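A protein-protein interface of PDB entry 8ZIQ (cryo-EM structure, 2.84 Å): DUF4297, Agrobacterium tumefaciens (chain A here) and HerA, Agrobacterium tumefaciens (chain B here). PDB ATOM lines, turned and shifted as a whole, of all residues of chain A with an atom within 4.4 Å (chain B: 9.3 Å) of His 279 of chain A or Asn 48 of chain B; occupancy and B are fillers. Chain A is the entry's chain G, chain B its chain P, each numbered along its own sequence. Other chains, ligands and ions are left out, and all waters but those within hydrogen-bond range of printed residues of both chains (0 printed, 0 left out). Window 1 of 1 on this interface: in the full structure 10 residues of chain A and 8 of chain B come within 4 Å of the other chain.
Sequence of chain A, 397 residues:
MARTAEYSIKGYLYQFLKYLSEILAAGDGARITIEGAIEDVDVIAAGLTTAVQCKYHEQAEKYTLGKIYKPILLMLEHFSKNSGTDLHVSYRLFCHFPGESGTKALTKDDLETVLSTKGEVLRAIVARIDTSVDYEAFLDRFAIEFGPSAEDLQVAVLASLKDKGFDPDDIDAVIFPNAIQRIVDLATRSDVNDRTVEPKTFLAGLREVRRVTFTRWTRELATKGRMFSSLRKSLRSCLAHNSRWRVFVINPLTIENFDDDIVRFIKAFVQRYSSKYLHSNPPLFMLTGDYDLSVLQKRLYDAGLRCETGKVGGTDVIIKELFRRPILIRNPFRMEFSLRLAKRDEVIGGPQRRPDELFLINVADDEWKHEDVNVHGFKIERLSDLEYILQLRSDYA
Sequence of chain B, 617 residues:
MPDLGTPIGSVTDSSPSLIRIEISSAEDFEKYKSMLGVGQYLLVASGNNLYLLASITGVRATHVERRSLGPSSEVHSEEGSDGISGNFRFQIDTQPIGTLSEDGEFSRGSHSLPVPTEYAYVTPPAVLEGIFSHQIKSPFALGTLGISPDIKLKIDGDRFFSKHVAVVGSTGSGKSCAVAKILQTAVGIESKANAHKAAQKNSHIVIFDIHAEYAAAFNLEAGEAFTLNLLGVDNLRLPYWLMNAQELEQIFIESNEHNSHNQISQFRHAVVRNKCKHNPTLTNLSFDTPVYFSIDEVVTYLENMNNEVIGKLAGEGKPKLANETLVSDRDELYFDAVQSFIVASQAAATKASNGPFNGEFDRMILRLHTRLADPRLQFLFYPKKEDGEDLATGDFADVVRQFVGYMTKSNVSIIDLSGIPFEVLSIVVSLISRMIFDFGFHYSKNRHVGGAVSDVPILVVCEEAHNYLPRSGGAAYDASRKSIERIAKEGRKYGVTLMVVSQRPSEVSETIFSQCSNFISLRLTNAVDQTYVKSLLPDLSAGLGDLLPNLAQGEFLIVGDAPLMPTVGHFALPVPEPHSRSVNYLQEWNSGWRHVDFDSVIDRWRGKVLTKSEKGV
Among the printed residues, pairs that only touch across the chains: Tyr 273 of chain A with Asn 48 of chain B (3.5 Å), Leu 278 of chain A with Val 115 of chain B (3.5 Å), Leu 278 of chain A with Pro 116 of chain B (3.8 Å), Leu 278 of chain A with Thr 117 of chain B (3.4 Å) and Leu 278 of chain A with Glu 118 of chain B (3.8 Å).
The backbone carbonyl oxygen (O) of Leu 239 of chain A lies close to the side-chain amide oxygen (OD1) of Asn 48 of chain B (3.0 Å).
The backbone NH of Asn 48 of chain B sits at hydrogen-bond distance from the backbone carbonyl oxygen of Ala 240 of chain A (3.2 Å).
O of His 241 of chain A lies close to OD1 of Asn 48 of chain B (3.1 Å).
The guanidinium group (NH1) of Arg 272 of chain A sits at hydrogen-bond distance from the side-chain amide oxygen (OD1) of Asn 49 of chain B.
ND2 of Asn 49 of chain B lies within hydrogen-bond range of OH of Tyr 273 of chain A, at 3.1 Å.
The side-chain amide nitrogen of Asn 48 of chain B lies within hydrogen-bond range of a ring nitrogen (NE2) of His 279 of chain A, at 3.3 Å.
Of the 17 printed residues of chain B, 6 touch a printed residue of chain A.
Printed residues of chain B that touch a printed residue of chain A: Asn 48, Asn 49, Val 115, Pro 116, Thr 117 and Glu 118.
Hydrophobic or aromatic side chains of chain B within 4 Å of the printed part of chain A: Val 115.
Along chain B the printed residues that touch a printed residue of chain A span positions 48 to 118.
Of the 15 printed residues of chain A, 7 touch a printed residue of chain B.
Hydrophobic or aromatic side chains of chain A that line the printed part of chain B: Tyr 273, Leu 278 and His 279.
Among the printed residues, 11 pairs touch across the chains.
Among the printed residues, no Asp or Glu carboxylate lies within 4 Å of a Lys or Arg side-chain nitrogen of the other chain.
Of chain B, only Asn 48 (3.3 Å) comes within 4 Å of His 279 of chain A.
Of chain A, only Leu 239, Ala 240, His 241, Tyr 273 and His 279 come within 4 Å of Asn 48 of chain B.
Of the printed residues of chain B, Leu 278 of chain A touches Val 115, Pro 116, Thr 117 and Glu 118.
Printed residues of chain A within 4 Å of Pro 116 of chain B: Leu 278.
Printed residues of chain A within 4 Å of Val 115 of chain B: Leu 278.
Of the printed residues of chain B, Arg 272 of chain A touches Asn 49 (2.8 Å).
The nearest residue of chain B that does not touch His 279 of chain A is Gly 47 of chain B (6.4 Å).
The nearest printed residue of chain A that does not touch Val 115 of chain B is Asn 242 of chain A (5.5 Å).
A ring nitrogen (NE2) of His 279 of chain A is in hydrogen-bond range of the side-chain amide oxygen (OD1) of Asn 242 of chain A, 3.4 Å away.
The backbone carbonyl oxygen of Tyr 273 of chain A is in hydrogen-bond range of a ring nitrogen (ND1) of His 279 of chain A (3.2 Å).
N of Ser 275 of chain A is in hydrogen-bond range of ND1 of His 279 of chain A (3.5 Å).
O of Ala 45 of chain B sits close to OE1 of Glu 118 of chain B (2.6 Å).
N of Val 115 of chain B lies within hydrogen-bond range of OE1 of Glu 118 of chain B.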
ATOM      1  N   LEU A 239       1.072   1.511  22.689  1.00  0.00           N
ATOM      2  CA  LEU A 239       0.552   2.367  23.739  1.00  0.00           C
ATOM      3  C   LEU A 239      -0.929   2.147  24.016  1.00  0.00           C
ATOM      4  O   LEU A 239      -1.421   2.593  25.056  1.00  0.00           O
ATOM      5  CB  LEU A 239       0.806   3.815  23.366  1.00  0.00           C
ATOM      6  CG  LEU A 239       2.241   4.299  23.504  1.00  0.00           C
ATOM      7  CD1 LEU A 239       2.333   5.716  23.096  1.00  0.00           C
ATOM      8  CD2 LEU A 239       2.787   4.139  24.879  1.00  0.00           C
ATOM      9  N   ALA A 240      -1.657   1.486  23.116  1.00  0.00           N
ATOM     10  CA  ALA A 240      -3.085   1.293  23.329  1.00  0.00           C
ATOM     11  C   ALA A 240      -3.370   0.381  24.513  1.00  0.00           C
ATOM     12  O   ALA A 240      -4.321   0.609  25.267  1.00  0.00           O
ATOM     13  CB  ALA A 240      -3.711   0.716  22.073  1.00  0.00           C
ATOM     14  N   HIS A 241      -2.569  -0.660  24.679  1.00  0.00           N
ATOM     15  CA  HIS A 241      -2.822  -1.682  25.683  1.00  0.00           C
ATOM     16  C   HIS A 241      -2.946  -1.103  27.087  1.00  0.00           C
ATOM     17  O   HIS A 241      -2.219  -0.180  27.462  1.00  0.00           O
ATOM     18  CB  HIS A 241      -1.707  -2.714  25.632  1.00  0.00           C
ATOM     19  CG  HIS A 241      -1.872  -3.725  24.546  1.00  0.00           C
ATOM     20  ND1 HIS A 241      -1.052  -3.771  23.444  1.00  0.00           N
ATOM     21  CD2 HIS A 241      -2.749  -4.744  24.405  1.00  0.00           C
ATOM     22  CE1 HIS A 241      -1.423  -4.766  22.662  1.00  0.00           C
ATOM     23  NE2 HIS A 241      -2.451  -5.373  23.222  1.00  0.00           N
ATOM     24  N   ASN A 242      -3.881  -1.648  27.868  1.00  0.00           N
ATOM     25  CA  ASN A 242      -4.064  -1.199  29.242  1.00  0.00           C
ATOM     26  C   ASN A 242      -2.976  -1.734  30.159  1.00  0.00           C
ATOM     27  O   ASN A 242      -2.441  -0.993  30.987  1.00  0.00           O
ATOM     28  CB  ASN A 242      -5.424  -1.619  29.789  1.00  0.00           C
ATOM     29  CG  ASN A 242      -6.572  -0.907  29.139  1.00  0.00           C
ATOM     30  OD1 ASN A 242      -6.868   0.232  29.471  1.00  0.00           O
ATOM     31  ND2 ASN A 242      -7.255  -1.587  28.238  1.00  0.00           N
ATOM     32  N   ARG A 272      -2.488   9.954  31.736  1.00  0.00           N
ATOM     33  CA  ARG A 272      -3.072   9.358  30.546  1.00  0.00           C
ATOM     34  C   ARG A 272      -2.967   7.839  30.563  1.00  0.00           C
ATOM     35  O   ARG A 272      -3.874   7.154  30.084  1.00  0.00           O
ATOM     36  CB  ARG A 272      -2.417   9.939  29.298  1.00  0.00           C
ATOM     37  CG  ARG A 272      -2.884   9.318  28.009  1.00  0.00           C
ATOM     38  CD  ARG A 272      -4.234   9.817  27.634  1.00  0.00           C
ATOM     39  NE  ARG A 272      -4.220  11.205  27.211  1.00  0.00           N
ATOM     40  CZ  ARG A 272      -3.919  11.601  25.988  1.00  0.00           C
ATOM     41  NH1 ARG A 272      -3.616  10.715  25.067  1.00  0.00           N
ATOM     42  NH2 ARG A 272      -3.933  12.881  25.684  1.00  0.00           N
ATOM     43  N   TYR A 273      -1.881   7.295  31.107  1.00  0.00           N
ATOM     44  CA  TYR A 273      -1.606   5.868  31.018  1.00  0.00           C
ATOM     45  C   TYR A 273      -1.654   5.096  32.331  1.00  0.00           C
ATOM     46  O   TYR A 273      -1.562   3.867  32.293  1.00  0.00           O
ATOM     47  CB  TYR A 273      -0.248   5.654  30.361  1.00  0.00           C
ATOM     48  CG  TYR A 273      -0.273   5.947  28.891  1.00  0.00           C
ATOM     49  CD1 TYR A 273      -0.822   5.059  28.002  1.00  0.00           C
ATOM     50  CD2 TYR A 273       0.249   7.117  28.395  1.00  0.00           C
ATOM     51  CE1 TYR A 273      -0.853   5.333  26.669  1.00  0.00           C
ATOM     52  CE2 TYR A 273       0.221   7.390  27.067  1.00  0.00           C
ATOM     53  CZ  TYR A 273      -0.330   6.506  26.213  1.00  0.00           C
ATOM     54  OH  TYR A 273      -0.343   6.814  24.886  1.00  0.00           O
ATOM     55  N   SER A 274      -1.764   5.752  33.486  1.00  0.00           N
ATOM     56  CA  SER A 274      -1.859   5.042  34.759  1.00  0.00           C
ATOM     57  C   SER A 274      -2.843   5.707  35.725  1.00  0.00           C
ATOM     58  O   SER A 274      -2.509   6.054  36.849  1.00  0.00           O
ATOM     59  CB  SER A 274      -0.490   4.918  35.406  1.00  0.00           C
ATOM     60  OG  SER A 274      -0.599   4.441  36.725  1.00  0.00           O
ATOM     61  N   SER A 275      -4.086   5.893  35.289  1.00  0.00           N
ATOM     62  CA  SER A 275      -5.111   6.498  36.127  1.00  0.00           C
ATOM     63  C   SER A 275      -6.425   5.745  36.010  1.00  0.00           C
ATOM     64  O   SER A 275      -7.481   6.320  35.747  1.00  0.00           O
ATOM     65  CB  SER A 275      -5.307   7.958  35.749  1.00  0.00           C
ATOM     66  OG  SER A 275      -6.274   8.084  34.724  1.00  0.00           O
ATOM     67  N   LYS A 276      -6.375   4.437  36.212  1.00  0.00           N
ATOM     68  CA  LYS A 276      -7.539   3.596  35.988  1.00  0.00           C
ATOM     69  C   LYS A 276      -7.346   2.272  36.706  1.00  0.00           C
ATOM     70  O   LYS A 276      -6.251   1.938  37.162  1.00  0.00           O
ATOM     71  CB  LYS A 276      -7.786   3.381  34.504  1.00  0.00           C
ATOM     72  CG  LYS A 276      -9.239   3.354  34.143  1.00  0.00           C
ATOM     73  CD  LYS A 276      -9.464   2.717  32.795  1.00  0.00           C
ATOM     74  CE  LYS A 276      -8.808   3.515  31.703  1.00  0.00           C
ATOM     75  NZ  LYS A 276      -8.893   2.848  30.397  1.00  0.00           N
ATOM     76  N   TYR A 277      -8.436   1.522  36.798  1.00  0.00           N
ATOM     77  CA  TYR A 277      -8.446   0.251  37.503  1.00  0.00           C
ATOM     78  C   TYR A 277      -7.871  -0.866  36.653  1.00  0.00           C
ATOM     79  O   TYR A 277      -7.313  -1.826  37.191  1.00  0.00           O
ATOM     80  CB  TYR A 277      -9.869  -0.079  37.922  1.00  0.00           C
ATOM     81  CG  TYR A 277     -10.067  -1.389  38.621  1.00  0.00           C
ATOM     82  CD1 TYR A 277      -9.810  -1.518  39.961  1.00  0.00           C
ATOM     83  CD2 TYR A 277     -10.561  -2.482  37.952  1.00  0.00           C
ATOM     84  CE1 TYR A 277     -10.007  -2.704  40.604  1.00  0.00           C
ATOM     85  CE2 TYR A 277     -10.757  -3.667  38.589  1.00  0.00           C
ATOM     86  CZ  TYR A 277     -10.480  -3.774  39.913  1.00  0.00           C
ATOM     87  OH  TYR A 277     -10.676  -4.960  40.557  1.00  0.00           O
ATOM     88  N   LEU A 278      -8.004  -0.761  35.340  1.00  0.00           N
ATOM     89  CA  LEU A 278      -7.474  -1.753  34.425  1.00  0.00           C
ATOM     90  C   LEU A 278      -5.995  -1.561  34.150  1.00  0.00           C
ATOM     91  O   LEU A 278      -5.415  -2.337  33.386  1.00  0.00           O
ATOM     92  CB  LEU A 278      -8.256  -1.709  33.121  1.00  0.00           C
ATOM     93  CG  LEU A 278      -9.705  -2.152  33.242  1.00  0.00           C
ATOM     94  CD1 LEU A 278     -10.538  -1.574  32.143  1.00  0.00           C
ATOM     95  CD2 LEU A 278      -9.797  -3.626  33.203  1.00  0.00           C
ATOM     96  N   HIS A 279      -5.383  -0.551  34.744  1.00  0.00           N
ATOM     97  CA  HIS A 279      -3.963  -0.274  34.592  1.00  0.00           C
ATOM     98  C   HIS A 279      -3.223  -0.911  35.758  1.00  0.00           C
ATOM     99  O   HIS A 279      -3.141  -0.342  36.846  1.00  0.00           O
ATOM    100  CB  HIS A 279      -3.724   1.224  34.512  1.00  0.00           C
ATOM    101  CG  HIS A 279      -4.221   1.844  33.249  1.00  0.00           C
ATOM    102  ND1 HIS A 279      -4.565   3.171  33.156  1.00  0.00           N
ATOM    103  CD2 HIS A 279      -4.419   1.320  32.019  1.00  0.00           C
ATOM    104  CE1 HIS A 279      -4.959   3.438  31.929  1.00  0.00           C
ATOM    105  NE2 HIS A 279      -4.881   2.332  31.217  1.00  0.00           N
ATOM    106  N   SER A 280      -2.671  -2.092  35.514  1.00  0.00           N
ATOM    107  CA  SER A 280      -2.207  -2.984  36.562  1.00  0.00           C
ATOM    108  C   SER A 280      -0.740  -2.780  36.906  1.00  0.00           C
ATOM    109  O   SER A 280      -0.383  -2.720  38.084  1.00  0.00           O
ATOM    110  CB  SER A 280      -2.454  -4.425  36.145  1.00  0.00           C
ATOM    111  OG  SER A 280      -1.820  -4.714  34.912  1.00  0.00           O
ATOM    112  N   ASN A 281       0.126  -2.711  35.897  1.00  0.00           N
ATOM    113  CA  ASN A 281       1.553  -2.577  36.120  1.00  0.00           C
ATOM    114  C   ASN A 281       1.998  -1.149  35.866  1.00  0.00           C
ATOM    115  O   ASN A 281       2.067  -0.730  34.702  1.00  0.00           O
ATOM    116  CB  ASN A 281       2.318  -3.536  35.224  1.00  0.00           C
ATOM    117  CG  ASN A 281       3.688  -3.837  35.742  1.00  0.00           C
ATOM    118  OD1 ASN A 281       4.282  -3.040  36.463  1.00  0.00           O
ATOM    119  ND2 ASN A 281       4.201  -5.001  35.390  1.00  0.00           N
ATOM    120  N   LEU A 328      -5.534  -2.167  44.629  1.00  0.00           N
ATOM    121  CA  LEU A 328      -6.446  -1.365  43.834  1.00  0.00           C
ATOM    122  C   LEU A 328      -7.860  -1.591  44.333  1.00  0.00           C
ATOM    123  O   LEU A 328      -8.333  -2.729  44.373  1.00  0.00           O
ATOM    124  CB  LEU A 328      -6.324  -1.733  42.362  1.00  0.00           C
ATOM    125  CG  LEU A 328      -5.097  -1.185  41.646  1.00  0.00           C
ATOM    126  CD1 LEU A 328      -3.855  -1.974  41.990  1.00  0.00           C
ATOM    127  CD2 LEU A 328      -5.294  -1.227  40.186  1.00  0.00           C
ATOM    128  N   VAL B  44     -17.770   6.063  25.149  1.00  0.00           N
ATOM    129  CA  VAL B  44     -17.331   4.981  26.016  1.00  0.00           C
ATOM    130  C   VAL B  44     -15.886   4.653  25.687  1.00  0.00           C
ATOM    131  O   VAL B  44     -15.537   4.466  24.517  1.00  0.00           O
ATOM    132  CB  VAL B  44     -18.214   3.736  25.864  1.00  0.00           C
ATOM    133  CG1 VAL B  44     -17.787   2.682  26.809  1.00  0.00           C
ATOM    134  CG2 VAL B  44     -19.636   4.063  26.104  1.00  0.00           C
ATOM    135  N   ALA B  45     -15.052   4.583  26.711  1.00  0.00           N
ATOM    136  CA  ALA B  45     -13.646   4.289  26.529  1.00  0.00           C
ATOM    137  C   ALA B  45     -13.404   2.811  26.277  1.00  0.00           C
ATOM    138  O   ALA B  45     -13.991   1.945  26.927  1.00  0.00           O
ATOM    139  CB  ALA B  45     -12.864   4.733  27.754  1.00  0.00           C
ATOM    140  N   SER B  46     -12.522   2.534  25.323  1.00  0.00           N
ATOM    141  CA  SER B  46     -12.126   1.180  24.947  1.00  0.00           C
ATOM    142  C   SER B  46     -10.631   1.241  24.662  1.00  0.00           C
ATOM    143  O   SER B  46     -10.214   1.424  23.517  1.00  0.00           O
ATOM    144  CB  SER B  46     -12.898   0.681  23.745  1.00  0.00           C
ATOM    145  OG  SER B  46     -12.336  -0.514  23.241  1.00  0.00           O
ATOM    146  N   GLY B  47      -9.834   1.079  25.704  1.00  0.00           N
ATOM    147  CA  GLY B  47      -8.402   1.184  25.580  1.00  0.00           C
ATOM    148  C   GLY B  47      -7.924   2.617  25.548  1.00  0.00           C
ATOM    149  O   GLY B  47      -8.695   3.573  25.485  1.00  0.00           O
ATOM    150  N   ASN B  48      -6.608   2.759  25.593  1.00  0.00           N
ATOM    151  CA  ASN B  48      -6.001   4.072  25.521  1.00  0.00           C
ATOM    152  C   ASN B  48      -6.158   4.647  24.124  1.00  0.00           C
ATOM    153  O   ASN B  48      -5.977   3.951  23.123  1.00  0.00           O
ATOM    154  CB  ASN B  48      -4.521   3.995  25.881  1.00  0.00           C
ATOM    155  CG  ASN B  48      -4.274   3.375  27.227  1.00  0.00           C
ATOM    156  OD1 ASN B  48      -3.289   2.676  27.423  1.00  0.00           O
ATOM    157  ND2 ASN B  48      -5.145   3.642  28.168  1.00  0.00           N
ATOM    158  N   ASN B  49      -6.491   5.930  24.064  1.00  0.00           N
ATOM    159  CA  ASN B  49      -6.490   6.681  22.816  1.00  0.00           C
ATOM    160  C   ASN B  49      -7.519   6.136  21.833  1.00  0.00           C
ATOM    161  O   ASN B  49      -7.245   5.955  20.647  1.00  0.00           O
ATOM    162  CB  ASN B  49      -5.094   6.703  22.212  1.00  0.00           C
ATOM    163  CG  ASN B  49      -4.067   7.223  23.166  1.00  0.00           C
ATOM    164  OD1 ASN B  49      -4.247   8.269  23.777  1.00  0.00           O
ATOM    165  ND2 ASN B  49      -2.974   6.512  23.287  1.00  0.00           N
ATOM    166  N   LEU B  50      -8.721   5.881  22.335  1.00  0.00           N
ATOM    167  CA  LEU B  50      -9.796   5.355  21.516  1.00  0.00           C
ATOM    168  C   LEU B  50     -11.102   5.543  22.262  1.00  0.00           C
ATOM    169  O   LEU B  50     -11.134   5.532  23.492  1.00  0.00           O
ATOM    170  CB  LEU B  50      -9.574   3.885  21.189  1.00  0.00           C
ATOM    171  CG  LEU B  50     -10.475   3.268  20.139  1.00  0.00           C
ATOM    172  CD1 LEU B  50     -10.191   3.865  18.812  1.00  0.00           C
ATOM    173  CD2 LEU B  50     -10.282   1.788  20.079  1.00  0.00           C
ATOM    174  N   TYR B  51     -12.179   5.708  21.499  1.00  0.00           N
ATOM    175  CA  TYR B  51     -13.503   5.917  22.060  1.00  0.00           C
ATOM    176  C   TYR B  51     -14.558   5.363  21.119  1.00  0.00           C
ATOM    177  O   TYR B  51     -14.361   5.299  19.906  1.00  0.00           O
ATOM    178  CB  TYR B  51     -13.799   7.390  22.315  1.00  0.00           C
ATOM    179  CG  TYR B  51     -12.993   8.046  23.392  1.00  0.00           C
ATOM    180  CD1 TYR B  51     -13.405   8.006  24.698  1.00  0.00           C
ATOM    181  CD2 TYR B  51     -11.841   8.739  23.099  1.00  0.00           C
ATOM    182  CE1 TYR B  51     -12.693   8.607  25.681  1.00  0.00           C
ATOM    183  CE2 TYR B  51     -11.118   9.344  24.082  1.00  0.00           C
ATOM    184  CZ  TYR B  51     -11.551   9.272  25.376  1.00  0.00           C
ATOM    185  OH  TYR B  51     -10.840   9.870  26.380  1.00  0.00           O
ATOM    186  N   THR B  99     -16.497   4.425  15.964  1.00  0.00           N
ATOM    187  CA  THR B  99     -15.276   4.669  16.708  1.00  0.00           C
ATOM    188  C   THR B  99     -14.737   6.053  16.387  1.00  0.00           C
ATOM    189  O   THR B  99     -14.864   6.547  15.267  1.00  0.00           O
ATOM    190  CB  THR B  99     -14.211   3.626  16.386  1.00  0.00           C
ATOM    191  OG1 THR B  99     -14.700   2.321  16.702  1.00  0.00           O
ATOM    192  CG2 THR B  99     -12.963   3.874  17.178  1.00  0.00           C
ATOM    193  N   LEU B 100     -14.139   6.667  17.394  1.00  0.00           N
ATOM    194  CA  LEU B 100     -13.532   7.984  17.315  1.00  0.00           C
ATOM    195  C   LEU B 100     -12.210   7.937  18.058  1.00  0.00           C
ATOM    196  O   LEU B 100     -12.163   7.511  19.214  1.00  0.00           O
ATOM    197  CB  LEU B 100     -14.432   9.054  17.909  1.00  0.00           C
ATOM    198  CG  LEU B 100     -13.861  10.454  17.879  1.00  0.00           C
ATOM    199  CD1 LEU B 100     -13.848  11.009  16.467  1.00  0.00           C
ATOM    200  CD2 LEU B 100     -14.638  11.302  18.792  1.00  0.00           C
ATOM    201  N   SER B 101     -11.146   8.359  17.394  1.00  0.00           N
ATOM    202  CA  SER B 101      -9.820   8.332  17.970  1.00  0.00           C
ATOM    203  C   SER B 101      -9.467   9.636  18.668  1.00  0.00           C
ATOM    204  O   SER B 101     -10.252  10.583  18.746  1.00  0.00           O
ATOM    205  CB  SER B 101      -8.784   8.033  16.900  1.00  0.00           C
ATOM    206  OG  SER B 101      -7.479   8.182  17.409  1.00  0.00           O
ATOM    207  N   GLU B 102      -8.250   9.664  19.195  1.00  0.00           N
ATOM    208  CA  GLU B 102      -7.807  10.804  19.971  1.00  0.00           C
ATOM    209  C   GLU B 102      -7.568  11.990  19.068  1.00  0.00           C
ATOM    210  O   GLU B 102      -7.905  13.130  19.413  1.00  0.00           O
ATOM    211  CB  GLU B 102      -6.534  10.430  20.725  1.00  0.00           C
ATOM    212  CG  GLU B 102      -5.868  11.555  21.440  1.00  0.00           C
ATOM    213  CD  GLU B 102      -6.798  12.307  22.346  1.00  0.00           C
ATOM    214  OE1 GLU B 102      -7.515  11.658  23.123  1.00  0.00           O
ATOM    215  OE2 GLU B 102      -6.856  13.550  22.232  1.00  0.00           O
ATOM    216  N   VAL B 115     -14.581  -3.340  27.854  1.00  0.00           N
ATOM    217  CA  VAL B 115     -14.516  -4.211  29.021  1.00  0.00           C
ATOM    218  C   VAL B 115     -15.152  -3.469  30.185  1.00  0.00           C
ATOM    219  O   VAL B 115     -15.138  -2.230  30.210  1.00  0.00           O
ATOM    220  CB  VAL B 115     -13.081  -4.644  29.352  1.00  0.00           C
ATOM    221  CG1 VAL B 115     -12.497  -5.427  28.230  1.00  0.00           C
ATOM    222  CG2 VAL B 115     -12.205  -3.444  29.674  1.00  0.00           C
ATOM    223  N   PRO B 116     -15.716  -4.167  31.160  1.00  0.00           N
ATOM    224  CA  PRO B 116     -16.286  -3.485  32.314  1.00  0.00           C
ATOM    225  C   PRO B 116     -15.235  -2.720  33.093  1.00  0.00           C
ATOM    226  O   PRO B 116     -14.026  -2.857  32.897  1.00  0.00           O
ATOM    227  CB  PRO B 116     -16.886  -4.626  33.119  1.00  0.00           C
ATOM    228  CG  PRO B 116     -17.207  -5.607  32.138  1.00  0.00           C
ATOM    229  CD  PRO B 116     -16.196  -5.548  31.083  1.00  0.00           C
ATOM    230  N   THR B 117     -15.733  -1.890  34.000  1.00  0.00           N
ATOM    231  CA  THR B 117     -14.927  -0.976  34.791  1.00  0.00           C
ATOM    232  C   THR B 117     -14.390   0.176  33.955  1.00  0.00           C
ATOM    233  O   THR B 117     -13.368   0.775  34.290  1.00  0.00           O
ATOM    234  CB  THR B 117     -13.785  -1.708  35.484  1.00  0.00           C
ATOM    235  OG1 THR B 117     -12.854  -2.201  34.512  1.00  0.00           O
ATOM    236  CG2 THR B 117     -14.336  -2.850  36.273  1.00  0.00           C
ATOM    237  N   GLU B 118     -15.079   0.491  32.864  1.00  0.00           N
ATOM    238  CA  GLU B 118     -14.665   1.520  31.928  1.00  0.00           C
ATOM    239  C   GLU B 118     -15.673   2.655  31.932  1.00  0.00           C
ATOM    240  O   GLU B 118     -16.885   2.429  31.976  1.00  0.00           O
ATOM    241  CB  GLU B 118     -14.495   0.966  30.518  1.00  0.00           C
ATOM    242  CG  GLU B 118     -13.140   0.358  30.256  1.00  0.00           C
ATOM    243  CD  GLU B 118     -13.014  -0.223  28.868  1.00  0.00           C
ATOM    244  OE1 GLU B 118     -14.051  -0.373  28.186  1.00  0.00           O
ATOM    245  OE2 GLU B 118     -11.875  -0.521  28.453  1.00  0.00           O
ATOM    246  N   TYR B 119     -15.157   3.873  31.880  1.00  0.00           N
ATOM    247  CA  TYR B 119     -15.928   5.080  32.089  1.00  0.00           C
ATOM    248  C   TYR B 119     -16.716   5.464  30.845  1.00  0.00           C
ATOM    249  O   TYR B 119     -16.371   5.103  29.719  1.00  0.00           O
ATOM    250  CB  TYR B 119     -15.012   6.224  32.507  1.00  0.00           C
ATOM    251  CG  TYR B 119     -14.453   6.100  33.899  1.00  0.00           C
ATOM    252  CD1 TYR B 119     -15.255   5.739  34.961  1.00  0.00           C
ATOM    253  CD2 TYR B 119     -13.125   6.362  34.154  1.00  0.00           C
ATOM    254  CE1 TYR B 119     -14.746   5.632  36.227  1.00  0.00           C
ATOM    255  CE2 TYR B 119     -12.611   6.257  35.418  1.00  0.00           C
ATOM    256  CZ  TYR B 119     -13.424   5.890  36.449  1.00  0.00           C
ATOM    257  OH  TYR B 119     -12.911   5.785  37.714  1.00  0.00           O
